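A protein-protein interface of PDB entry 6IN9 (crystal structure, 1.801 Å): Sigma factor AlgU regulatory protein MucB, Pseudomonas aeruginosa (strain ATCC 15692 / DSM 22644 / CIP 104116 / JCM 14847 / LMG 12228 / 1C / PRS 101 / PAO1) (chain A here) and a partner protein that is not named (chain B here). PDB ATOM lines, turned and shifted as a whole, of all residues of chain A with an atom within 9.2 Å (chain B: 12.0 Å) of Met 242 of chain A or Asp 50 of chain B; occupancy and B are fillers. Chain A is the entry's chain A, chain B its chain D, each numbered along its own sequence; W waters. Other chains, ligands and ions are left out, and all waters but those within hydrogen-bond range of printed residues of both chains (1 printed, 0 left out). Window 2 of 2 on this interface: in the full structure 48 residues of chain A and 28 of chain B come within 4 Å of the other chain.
The side-chain carboxylate (OD2) of Asp 50 of chain B is in hydrogen-bond range of the backbone NH (N) of Gly 244 of chain A (3.0 Å).
A ring nitrogen (NE2) of His 54 of chain B sits at hydrogen-bond distance from the backbone carbonyl oxygen (O) of Gly 244 of chain A, 2.9 Å away.
N of Arg 247 of chain A sits at hydrogen-bond distance from O of Ile 43 of chain B, 2.6 Å away.
N of Leu 238 of chain A sits at hydrogen-bond distance from O of Gly 266 of chain A.
The backbone carbonyl oxygen (O) of Ala 246 of chain A is in hydrogen-bond range of the backbone NH (N) of Ser 257 of chain A (2.9 Å).
The backbone NH (N) of Arg 259 of chain A lies within hydrogen-bond range of the side-chain sulfur (SD) of Met 268 of chain A (3.7 Å).
The side-chain hydroxyl (OG) of Ser 47 of chain B is in hydrogen-bond range of the backbone NH (N) of Asp 50 of chain B (3.1 Å).
The backbone carbonyl oxygen of Trp 53 of chain B lies within hydrogen-bond range of the guanidinium group of Arg 57 of chain B (2.9 Å).
CD2 of Leu 238 of chain A touches CZ2 of Trp 53 of chain B, 3.7 Å away.
OD1 of Asp 50 of chain B touches O of Met 242 of chain A, at 3.6 Å.
Asp 50 of chain B touches Val 243 of chain A (OD1 to CA, 3.6 Å).
Val 243 of chain A touches Trp 53 of chain B (CG1 to CE3, 3.7 Å).
Ala 246 of chain A touches Ile 43 of chain B.
Ala 246 of chain A touches His 54 of chain B.
Ala 246 of chain A touches Leu 58 of chain B.
Ser 257 of chain A touches His 54 of chain B (CB to CE1, 3.5 Å).
CD2 of Leu 58 of chain B touches OG of Ser 257 of chain A, 3.1 Å away.
Met 268 of chain A touches Trp 53 of chain B.
Met 242 of chain A touches just one residue of chain B: Asp 50.
Asp 50 of chain B touches just these residues of chain A: Met 242 (3.6 Å), Val 243 (3.6 Å) and Gly 244 (3.0 Å).
No residue of chain B comes within 4 Å of Ala 241 of chain A.
Val 243 of chain A touches just these residues of chain B: Asp 50, Trp 53 and His 54.
Gly 244 of chain A touches just these residues of chain B: Asp 50 (3.0 Å) and His 54 (2.9 Å).
No residue of chain A comes within 4 Å of Ser 47 of chain B.
No residue of chain A comes within 4 Å of Ser 49 of chain B.
No residue of chain A comes within 4 Å of Thr 51 of chain B.
Of the printed residues of chain A, Val 42 of chain B touches Arg 247 (3.8 Å).
Printed residues of chain A within 4 Å of Ile 43 of chain B: Ala 246 and Arg 247.
Of the printed residues of chain B, Met 268 of chain A touches Trp 53 and His 54.
Of the printed residues of chain B, Leu 238 of chain A touches Trp 53.
Tyr 61 of chain B touches none of the printed residues of chain A.
Arg 259 of chain A touches none of the printed residues of chain B.
The nearest residue of chain B that does not touch Met 242 of chain A is Ser 49 of chain B (5.3 Å).
The nearest printed residue of chain B that does not touch Met 268 of chain A is Arg 57 of chain B (6.6 Å).
Printed residues of chain A that touch a printed residue of chain B: Leu 238, Met 242, Val 243, Gly 244, Ala 246, Arg 247, Ser 257 and Met 268.
Hydrophobic or aromatic side chains of chain A within 4 Å of the printed part of chain B: Leu 238, Val 243, Ala 246 and Met 268.
Among the printed residues, no Asp or Glu carboxylate lies within 4 Å of a Lys or Arg side-chain nitrogen of the other chain.
Water W1 lies within hydrogen-bond range of a ring nitrogen (ND1) of His 54 of chain B (3.0 Å) and the side-chain hydroxyl of Ser 257 of chain A (3.3 Å).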
ATOM      1  N   LEU A 238      -9.023  20.967  14.843  1.00  0.00           N
ATOM      2  CA  LEU A 238      -9.943  20.127  15.593  1.00  0.00           C
ATOM      3  C   LEU A 238     -11.112  19.619  14.759  1.00  0.00           C
ATOM      4  O   LEU A 238     -11.774  18.666  15.180  1.00  0.00           O
ATOM      5  CB  LEU A 238     -10.497  20.897  16.797  1.00  0.00           C
ATOM      6  CG  LEU A 238      -9.455  21.096  17.911  1.00  0.00           C
ATOM      7  CD1 LEU A 238      -9.990  22.052  18.958  1.00  0.00           C
ATOM      8  CD2 LEU A 238      -9.132  19.746  18.522  1.00  0.00           C
ATOM      9  N   HIS A 239     -11.372  20.212  13.597  1.00  0.00           N
ATOM     10  CA  HIS A 239     -12.480  19.755  12.747  1.00  0.00           C
ATOM     11  C   HIS A 239     -13.793  19.715  13.518  1.00  0.00           C
ATOM     12  O   HIS A 239     -14.552  18.749  13.415  1.00  0.00           O
ATOM     13  CB  HIS A 239     -12.198  18.364  12.168  1.00  0.00           C
ATOM     14  CG  HIS A 239     -11.089  18.328  11.165  1.00  0.00           C
ATOM     15  ND1 HIS A 239     -11.278  18.647   9.837  1.00  0.00           N
ATOM     16  CD2 HIS A 239      -9.787  17.983  11.288  1.00  0.00           C
ATOM     17  CE1 HIS A 239     -10.135  18.511   9.187  1.00  0.00           C
ATOM     18  NE2 HIS A 239      -9.213  18.116  10.047  1.00  0.00           N
ATOM     19  N   GLY A 240     -14.034  20.729  14.345  1.00  0.00           N
ATOM     20  CA  GLY A 240     -15.264  20.821  15.095  1.00  0.00           C
ATOM     21  C   GLY A 240     -15.359  19.958  16.334  1.00  0.00           C
ATOM     22  O   GLY A 240     -16.388  20.015  17.021  1.00  0.00           O
ATOM     23  N   ALA A 241     -14.330  19.171  16.653  1.00  0.00           N
ATOM     24  CA  ALA A 241     -14.380  18.295  17.818  1.00  0.00           C
ATOM     25  C   ALA A 241     -14.322  19.082  19.127  1.00  0.00           C
ATOM     26  O   ALA A 241     -13.685  20.133  19.224  1.00  0.00           O
ATOM     27  CB  ALA A 241     -13.230  17.286  17.784  1.00  0.00           C
ATOM     28  N   MET A 242     -14.992  18.542  20.150  1.00  0.00           N
ATOM     29  CA  MET A 242     -14.953  19.067  21.515  1.00  0.00           C
ATOM     30  C   MET A 242     -13.809  18.373  22.231  1.00  0.00           C
ATOM     31  O   MET A 242     -13.959  17.275  22.767  1.00  0.00           O
ATOM     32  CB  MET A 242     -16.262  18.813  22.255  1.00  0.00           C
ATOM     33  CG  MET A 242     -17.511  19.105  21.473  1.00  0.00           C
ATOM     34  SD  MET A 242     -17.866  20.856  21.580  1.00  0.00           S
ATOM     35  CE  MET A 242     -17.084  21.482  20.091  1.00  0.00           C
ATOM     36  N   VAL A 243     -12.647  19.007  22.227  1.00  0.00           N
ATOM     37  CA  VAL A 243     -11.496  18.534  22.979  1.00  0.00           C
ATOM     38  C   VAL A 243     -11.081  19.667  23.903  1.00  0.00           C
ATOM     39  O   VAL A 243     -10.981  20.816  23.463  1.00  0.00           O
ATOM     40  CB  VAL A 243     -10.337  18.119  22.055  1.00  0.00           C
ATOM     41  CG1 VAL A 243      -9.169  17.593  22.882  1.00  0.00           C
ATOM     42  CG2 VAL A 243     -10.801  17.075  21.051  1.00  0.00           C
ATOM     43  N   GLY A 244     -10.873  19.350  25.183  1.00  0.00           N
ATOM     44  CA  GLY A 244     -10.599  20.351  26.191  1.00  0.00           C
ATOM     45  C   GLY A 244      -9.116  20.515  26.493  1.00  0.00           C
ATOM     46  O   GLY A 244      -8.243  20.014  25.781  1.00  0.00           O
ATOM     47  N   ASP A 245      -8.848  21.246  27.578  1.00  0.00           N
ATOM     48  CA  ASP A 245      -7.488  21.558  28.016  1.00  0.00           C
ATOM     49  C   ASP A 245      -6.681  20.299  28.330  1.00  0.00           C
ATOM     50  O   ASP A 245      -7.222  19.265  28.729  1.00  0.00           O
ATOM     51  CB  ASP A 245      -7.500  22.407  29.296  1.00  0.00           C
ATOM     52  CG  ASP A 245      -8.171  23.755  29.135  1.00  0.00           C
ATOM     53  OD1 ASP A 245      -8.379  24.214  27.994  1.00  0.00           O
ATOM     54  OD2 ASP A 245      -8.463  24.369  30.191  1.00  0.00           O
ATOM     55  N   ALA A 246      -5.357  20.424  28.228  1.00  0.00           N
ATOM     56  CA  ALA A 246      -4.464  19.417  28.796  1.00  0.00           C
ATOM     57  C   ALA A 246      -3.223  20.109  29.334  1.00  0.00           C
ATOM     58  O   ALA A 246      -2.874  21.220  28.919  1.00  0.00           O
ATOM     59  CB  ALA A 246      -4.069  18.354  27.774  1.00  0.00           C
ATOM     60  N   ARG A 247      -2.562  19.456  30.281  1.00  0.00           N
ATOM     61  CA  ARG A 247      -1.289  19.987  30.733  1.00  0.00           C
ATOM     62  C   ARG A 247      -0.413  18.843  31.209  1.00  0.00           C
ATOM     63  O   ARG A 247      -0.895  17.760  31.550  1.00  0.00           O
ATOM     64  CB  ARG A 247      -1.457  21.043  31.834  1.00  0.00           C
ATOM     65  CG  ARG A 247      -2.001  20.506  33.130  1.00  0.00           C
ATOM     66  CD  ARG A 247      -2.007  21.574  34.224  1.00  0.00           C
ATOM     67  NE  ARG A 247      -1.645  20.991  35.513  1.00  0.00           N
ATOM     68  CZ  ARG A 247      -2.471  20.271  36.266  1.00  0.00           C
ATOM     69  NH1 ARG A 247      -3.714  20.047  35.858  1.00  0.00           N
ATOM     70  NH2 ARG A 247      -2.052  19.773  37.422  1.00  0.00           N
ATOM     71  N   SER A 257      -2.006  22.649  26.575  1.00  0.00           N
ATOM     72  CA  SER A 257      -2.830  22.647  25.371  1.00  0.00           C
ATOM     73  C   SER A 257      -4.145  23.332  25.691  1.00  0.00           C
ATOM     74  O   SER A 257      -4.802  22.987  26.682  1.00  0.00           O
ATOM     75  CB  SER A 257      -3.096  21.232  24.863  1.00  0.00           C
ATOM     76  OG  SER A 257      -1.894  20.620  24.443  1.00  0.00           O
ATOM     77  N   ARG A 259      -7.735  24.984  23.633  1.00  0.00           N
ATOM     78  CA  ARG A 259      -8.477  25.140  22.386  1.00  0.00           C
ATOM     79  C   ARG A 259      -8.552  26.611  21.990  1.00  0.00           C
ATOM     80  O   ARG A 259      -8.675  27.502  22.838  1.00  0.00           O
ATOM     81  CB  ARG A 259      -9.885  24.552  22.530  1.00  0.00           C
ATOM     82  CG  ARG A 259     -10.836  24.828  21.347  1.00  0.00           C
ATOM     83  CD  ARG A 259     -12.245  24.250  21.589  1.00  0.00           C
ATOM     84  NE  ARG A 259     -13.054  24.220  20.366  1.00  0.00           N
ATOM     85  CZ  ARG A 259     -13.739  25.262  19.897  1.00  0.00           C
ATOM     86  NH1 ARG A 259     -13.723  26.435  20.537  1.00  0.00           N
ATOM     87  NH2 ARG A 259     -14.448  25.140  18.783  1.00  0.00           N
ATOM     88  N   GLY A 265     -13.191  25.536  12.280  1.00  0.00           N
ATOM     89  CA  GLY A 265     -13.372  24.311  13.031  1.00  0.00           C
ATOM     90  C   GLY A 265     -12.666  24.251  14.366  1.00  0.00           C
ATOM     91  O   GLY A 265     -12.725  23.210  15.029  1.00  0.00           O
ATOM     92  N   GLY A 266     -12.002  25.323  14.780  1.00  0.00           N
ATOM     93  CA  GLY A 266     -11.242  25.310  16.016  1.00  0.00           C
ATOM     94  C   GLY A 266      -9.868  24.691  15.869  1.00  0.00           C
ATOM     95  O   GLY A 266      -9.643  23.844  14.995  1.00  0.00           O
ATOM     96  N   MET A 268      -6.360  23.224  18.306  1.00  0.00           N
ATOM     97  CA  MET A 268      -5.723  22.975  19.589  1.00  0.00           C
ATOM     98  C   MET A 268      -4.358  23.635  19.532  1.00  0.00           C
ATOM     99  O   MET A 268      -3.590  23.373  18.601  1.00  0.00           O
ATOM    100  CB  MET A 268      -5.600  21.475  19.868  1.00  0.00           C
ATOM    101  CG  MET A 268      -5.055  21.129  21.262  1.00  0.00           C
ATOM    102  SD  MET A 268      -6.117  21.777  22.577  1.00  0.00           S
ATOM    103  CE  MET A 268      -7.608  20.849  22.223  1.00  0.00           C
ATOM    104  N   GLN B  41       2.096  11.161  30.381  1.00  0.00           N
ATOM    105  CA  GLN B  41       2.165  12.120  31.476  1.00  0.00           C
ATOM    106  C   GLN B  41       1.044  13.151  31.375  1.00  0.00           C
ATOM    107  O   GLN B  41       1.106  14.211  32.003  1.00  0.00           O
ATOM    108  CB  GLN B  41       3.515  12.844  31.483  1.00  0.00           C
ATOM    109  CG  GLN B  41       4.706  12.000  31.075  1.00  0.00           C
ATOM    110  CD  GLN B  41       5.254  12.395  29.713  1.00  0.00           C
ATOM    111  OE1 GLN B  41       4.617  13.142  28.966  1.00  0.00           O
ATOM    112  NE2 GLN B  41       6.442  11.899  29.387  1.00  0.00           N
ATOM    113  N   VAL B  42       0.023  12.840  30.584  1.00  0.00           N
ATOM    114  CA  VAL B  42      -0.946  13.848  30.169  1.00  0.00           C
ATOM    115  C   VAL B  42      -1.948  14.084  31.289  1.00  0.00           C
ATOM    116  O   VAL B  42      -2.682  13.172  31.685  1.00  0.00           O
ATOM    117  CB  VAL B  42      -1.650  13.438  28.869  1.00  0.00           C
ATOM    118  CG1 VAL B  42      -2.731  14.455  28.512  1.00  0.00           C
ATOM    119  CG2 VAL B  42      -0.628  13.320  27.745  1.00  0.00           C
ATOM    120  N   ILE B  43      -1.975  15.307  31.800  1.00  0.00           N
ATOM    121  CA  ILE B  43      -2.944  15.693  32.810  1.00  0.00           C
ATOM    122  C   ILE B  43      -3.976  16.635  32.214  1.00  0.00           C
ATOM    123  O   ILE B  43      -3.710  17.821  32.003  1.00  0.00           O
ATOM    124  CB  ILE B  43      -2.275  16.351  34.032  1.00  0.00           C
ATOM    125  CG1 ILE B  43      -1.366  15.355  34.748  1.00  0.00           C
ATOM    126  CG2 ILE B  43      -3.335  16.897  34.983  1.00  0.00           C
ATOM    127  CD1 ILE B  43       0.105  15.648  34.595  1.00  0.00           C
ATOM    128  N   THR B  44      -5.144  16.117  31.879  1.00  0.00           N
ATOM    129  CA  THR B  44      -5.438  14.705  31.671  1.00  0.00           C
ATOM    130  C   THR B  44      -6.474  14.842  30.500  1.00  0.00           C
ATOM    131  O   THR B  44      -6.279  14.225  29.449  1.00  0.00           O
ATOM    132  CB  THR B  44      -5.959  13.915  32.982  1.00  0.00           C
ATOM    133  OG1 THR B  44      -5.245  14.326  34.159  1.00  0.00           O
ATOM    134  CG2 THR B  44      -5.874  12.402  32.824  1.00  0.00           C
ATOM    135  N   ASN B  45      -7.556  15.634  30.675  1.00  0.00           N
ATOM    136  CA  ASN B  45      -8.062  15.898  32.027  1.00  0.00           C
ATOM    137  C   ASN B  45      -9.493  15.663  32.274  1.00  0.00           C
ATOM    138  O   ASN B  45     -10.347  16.530  32.066  1.00  0.00           O
ATOM    139  CB  ASN B  45      -7.775  17.282  32.558  1.00  0.00           C
ATOM    140  CG  ASN B  45      -7.893  17.297  34.078  1.00  0.00           C
ATOM    141  OD1 ASN B  45      -8.819  16.726  34.660  1.00  0.00           O
ATOM    142  ND2 ASN B  45      -6.830  17.729  34.717  1.00  0.00           N
ATOM    143  N   SER B  46      -9.684  14.507  32.899  1.00  0.00           N
ATOM    144  CA  SER B  46     -10.898  13.999  33.505  1.00  0.00           C
ATOM    145  C   SER B  46     -11.785  13.356  32.476  1.00  0.00           C
ATOM    146  O   SER B  46     -12.727  12.659  32.845  1.00  0.00           O
ATOM    147  CB  SER B  46     -11.695  15.086  34.241  1.00  0.00           C
ATOM    148  OG  SER B  46     -12.213  16.057  33.346  1.00  0.00           O
ATOM    149  N   SER B  47     -11.523  13.566  31.198  1.00  0.00           N
ATOM    150  CA  SER B  47     -12.340  13.033  30.126  1.00  0.00           C
ATOM    151  C   SER B  47     -11.519  11.991  29.382  1.00  0.00           C
ATOM    152  O   SER B  47     -10.464  12.310  28.821  1.00  0.00           O
ATOM    153  CB  SER B  47     -12.790  14.157  29.197  1.00  0.00           C
ATOM    154  OG  SER B  47     -13.212  13.636  27.955  1.00  0.00           O
ATOM    155  N   SER B  48     -11.989  10.743  29.403  1.00  0.00           N
ATOM    156  CA  SER B  48     -11.280   9.686  28.696  1.00  0.00           C
ATOM    157  C   SER B  48     -11.212   9.967  27.201  1.00  0.00           C
ATOM    158  O   SER B  48     -10.255   9.557  26.537  1.00  0.00           O
ATOM    159  CB  SER B  48     -11.947   8.336  28.962  1.00  0.00           C
ATOM    160  OG  SER B  48     -11.639   7.878  30.266  1.00  0.00           O
ATOM    161  N   SER B  49     -12.210  10.664  26.656  1.00  0.00           N
ATOM    162  CA  SER B  49     -12.115  11.098  25.267  1.00  0.00           C
ATOM    163  C   SER B  49     -10.965  12.082  25.083  1.00  0.00           C
ATOM    164  O   SER B  49     -10.199  11.981  24.118  1.00  0.00           O
ATOM    165  CB  SER B  49     -13.438  11.718  24.813  1.00  0.00           C
ATOM    166  OG  SER B  49     -13.799  12.822  25.626  1.00  0.00           O
ATOM    167  N   ASP B  50     -10.810  13.025  26.016  1.00  0.00           N
ATOM    168  CA  ASP B  50      -9.747  14.013  25.877  1.00  0.00           C
ATOM    169  C   ASP B  50      -8.378  13.433  26.201  1.00  0.00           C
ATOM    170  O   ASP B  50      -7.379  13.855  25.607  1.00  0.00           O
ATOM    171  CB  ASP B  50     -10.028  15.230  26.756  1.00  0.00           C
ATOM    172  CG  ASP B  50     -11.210  16.032  26.267  1.00  0.00           C
ATOM    173  OD1 ASP B  50     -11.752  15.695  25.191  1.00  0.00           O
ATOM    174  OD2 ASP B  50     -11.592  17.004  26.954  1.00  0.00           O
ATOM    175  N   THR B  51      -8.301  12.477  27.131  1.00  0.00           N
ATOM    176  CA  THR B  51      -7.008  11.872  27.443  1.00  0.00           C
ATOM    177  C   THR B  51      -6.471  11.091  26.250  1.00  0.00           C
ATOM    178  O   THR B  51      -5.300  11.230  25.878  1.00  0.00           O
ATOM    179  CB  THR B  51      -7.120  10.975  28.678  1.00  0.00           C
ATOM    180  OG1 THR B  51      -7.048  11.785  29.859  1.00  0.00           O
ATOM    181  CG2 THR B  51      -5.990   9.942  28.706  1.00  0.00           C
ATOM    182  N   ARG B  52      -7.327  10.285  25.618  1.00  0.00           N
ATOM    183  CA  ARG B  52      -6.904   9.517  24.451  1.00  0.00           C
ATOM    184  C   ARG B  52      -6.452  10.433  23.318  1.00  0.00           C
ATOM    185  O   ARG B  52      -5.461  10.148  22.635  1.00  0.00           O
ATOM    186  CB  ARG B  52      -8.046   8.604  23.996  1.00  0.00           C
ATOM    187  CG  ARG B  52      -7.781   7.808  22.728  1.00  0.00           C
ATOM    188  CD  ARG B  52      -8.967   6.901  22.409  1.00  0.00           C
ATOM    189  NE  ARG B  52      -8.629   5.481  22.507  1.00  0.00           N
ATOM    190  CZ  ARG B  52      -8.932   4.695  23.538  1.00  0.00           C
ATOM    191  NH1 ARG B  52      -9.586   5.180  24.587  1.00  0.00           N
ATOM    192  NH2 ARG B  52      -8.576   3.415  23.525  1.00  0.00           N
ATOM    193  N   TRP B  53      -7.162  11.545  23.116  1.00  0.00           N
ATOM    194  CA  TRP B  53      -6.792  12.489  22.067  1.00  0.00           C
ATOM    195  C   TRP B  53      -5.430  13.122  22.348  1.00  0.00           C
ATOM    196  O   TRP B  53      -4.550  13.145  21.479  1.00  0.00           O
ATOM    197  CB  TRP B  53      -7.878  13.553  21.939  1.00  0.00           C
ATOM    198  CG  TRP B  53      -7.822  14.348  20.681  1.00  0.00           C
ATOM    199  CD1 TRP B  53      -8.529  14.126  19.523  1.00  0.00           C
ATOM    200  CD2 TRP B  53      -7.023  15.506  20.445  1.00  0.00           C
ATOM    201  NE1 TRP B  53      -8.210  15.083  18.586  1.00  0.00           N
ATOM    202  CE2 TRP B  53      -7.287  15.938  19.129  1.00  0.00           C
ATOM    203  CE3 TRP B  53      -6.106  16.221  21.219  1.00  0.00           C
ATOM    204  CZ2 TRP B  53      -6.666  17.052  18.575  1.00  0.00           C
ATOM    205  CZ3 TRP B  53      -5.498  17.319  20.668  1.00  0.00           C
ATOM    206  CH2 TRP B  53      -5.773  17.721  19.357  1.00  0.00           C
ATOM    207  N   HIS B  54      -5.231  13.635  23.563  1.00  0.00           N
ATOM    208  CA  HIS B  54      -3.975  14.307  23.874  1.00  0.00           C
ATOM    209  C   HIS B  54      -2.807  13.332  24.011  1.00  0.00           C
ATOM    210  O   HIS B  54      -1.666  13.697  23.691  1.00  0.00           O
ATOM    211  CB  HIS B  54      -4.126  15.124  25.155  1.00  0.00           C
ATOM    212  CG  HIS B  54      -4.873  16.408  24.964  1.00  0.00           C
ATOM    213  ND1 HIS B  54      -4.365  17.457  24.227  1.00  0.00           N
ATOM    214  CD2 HIS B  54      -6.069  16.827  25.444  1.00  0.00           C
ATOM    215  CE1 HIS B  54      -5.225  18.463  24.243  1.00  0.00           C
ATOM    216  NE2 HIS B  54      -6.263  18.109  24.983  1.00  0.00           N
ATOM    217  N   GLU B  55      -3.058  12.101  24.479  1.00  0.00           N
ATOM    218  CA  GLU B  55      -1.951  11.180  24.716  1.00  0.00           C
ATOM    219  C   GLU B  55      -1.273  10.739  23.425  1.00  0.00           C
ATOM    220  O   GLU B  55      -0.119  10.308  23.467  1.00  0.00           O
ATOM    221  CB  GLU B  55      -2.426   9.958  25.521  1.00  0.00           C
ATOM    222  CG  GLU B  55      -3.321   8.968  24.776  1.00  0.00           C
ATOM    223  CD  GLU B  55      -3.772   7.814  25.676  1.00  0.00           C
ATOM    224  OE1 GLU B  55      -3.720   7.981  26.916  1.00  0.00           O
ATOM    225  OE2 GLU B  55      -4.160   6.746  25.148  1.00  0.00           O
ATOM    226  N   GLN B  56      -1.940  10.862  22.280  1.00  0.00           N
ATOM    227  CA  GLN B  56      -1.327  10.509  21.007  1.00  0.00           C
ATOM    228  C   GLN B  56      -0.514  11.641  20.396  1.00  0.00           C
ATOM    229  O   GLN B  56       0.153  11.427  19.372  1.00  0.00           O
ATOM    230  CB  GLN B  56      -2.406  10.088  20.011  1.00  0.00           C
ATOM    231  CG  GLN B  56      -3.039   8.756  20.311  1.00  0.00           C
ATOM    232  CD  GLN B  56      -3.959   8.326  19.194  1.00  0.00           C
ATOM    233  OE1 GLN B  56      -5.126   8.707  19.164  1.00  0.00           O
ATOM    234  NE2 GLN B  56      -3.433   7.543  18.257  1.00  0.00           N
ATOM    235  N   ARG B  57      -0.571  12.833  20.979  1.00  0.00           N
ATOM    236  CA  ARG B  57       0.019  14.032  20.401  1.00  0.00           C
ATOM    237  C   ARG B  57       1.036  14.686  21.321  1.00  0.00           C
ATOM    238  O   ARG B  57       2.169  14.943  20.896  1.00  0.00           O
ATOM    239  CB  ARG B  57      -1.095  15.041  20.060  1.00  0.00           C
ATOM    240  CG  ARG B  57      -1.967  14.593  18.888  1.00  0.00           C
ATOM    241  CD  ARG B  57      -3.301  15.275  18.903  1.00  0.00           C
ATOM    242  NE  ARG B  57      -4.078  14.962  17.705  1.00  0.00           N
ATOM    243  CZ  ARG B  57      -4.919  13.938  17.593  1.00  0.00           C
ATOM    244  NH1 ARG B  57      -5.113  13.101  18.606  1.00  0.00           N
ATOM    245  NH2 ARG B  57      -5.581  13.755  16.458  1.00  0.00           N
ATOM    246  N   LEU B  58       0.653  14.975  22.568  1.00  0.00           N
ATOM    247  CA  LEU B  58       1.528  15.732  23.464  1.00  0.00           C
ATOM    248  C   LEU B  58       2.905  15.110  23.654  1.00  0.00           C
ATOM    249  O   LEU B  58       3.893  15.866  23.628  1.00  0.00           O
ATOM    250  CB  LEU B  58       0.871  15.914  24.837  1.00  0.00           C
ATOM    251  CG  LEU B  58      -0.328  16.834  24.961  1.00  0.00           C
ATOM    252  CD1 LEU B  58      -0.617  17.051  26.440  1.00  0.00           C
ATOM    253  CD2 LEU B  58      -0.041  18.139  24.253  1.00  0.00           C
ATOM    254  N   PRO B  59       3.052  13.801  23.877  1.00  0.00           N
ATOM    255  CA  PRO B  59       4.408  13.253  24.025  1.00  0.00           C
ATOM    256  C   PRO B  59       5.269  13.496  22.811  1.00  0.00           C
ATOM    257  O   PRO B  59       6.478  13.715  22.958  1.00  0.00           O
ATOM    258  CB  PRO B  59       4.157  11.751  24.250  1.00  0.00           C
ATOM    259  CG  PRO B  59       2.783  11.697  24.839  1.00  0.00           C
ATOM    260  CD  PRO B  59       2.025  12.765  24.097  1.00  0.00           C
ATOM    261  N   TYR B  61       4.987  16.107  20.530  1.00  0.00           N
ATOM    262  CA  TYR B  61       5.356  17.520  20.461  1.00  0.00           C
ATOM    263  C   TYR B  61       6.402  17.860  21.515  1.00  0.00           C
ATOM    264  O   TYR B  61       7.308  18.665  21.260  1.00  0.00           O
ATOM    265  CB  TYR B  61       4.109  18.398  20.626  1.00  0.00           C
ATOM    266  CG  TYR B  61       3.079  18.182  19.522  1.00  0.00           C
ATOM    267  CD1 TYR B  61       3.474  17.757  18.256  1.00  0.00           C
ATOM    268  CD2 TYR B  61       1.724  18.392  19.748  1.00  0.00           C
ATOM    269  CE1 TYR B  61       2.539  17.552  17.231  1.00  0.00           C
ATOM    270  CE2 TYR B  61       0.783  18.204  18.725  1.00  0.00           C
ATOM    271  CZ  TYR B  61       1.197  17.781  17.479  1.00  0.00           C
ATOM    272  OH  TYR B  61       0.260  17.582  16.465  1.00  0.00           O
HETATM  273  O   HOH W   1      -2.412  18.301  22.115  1.00  0.00           O
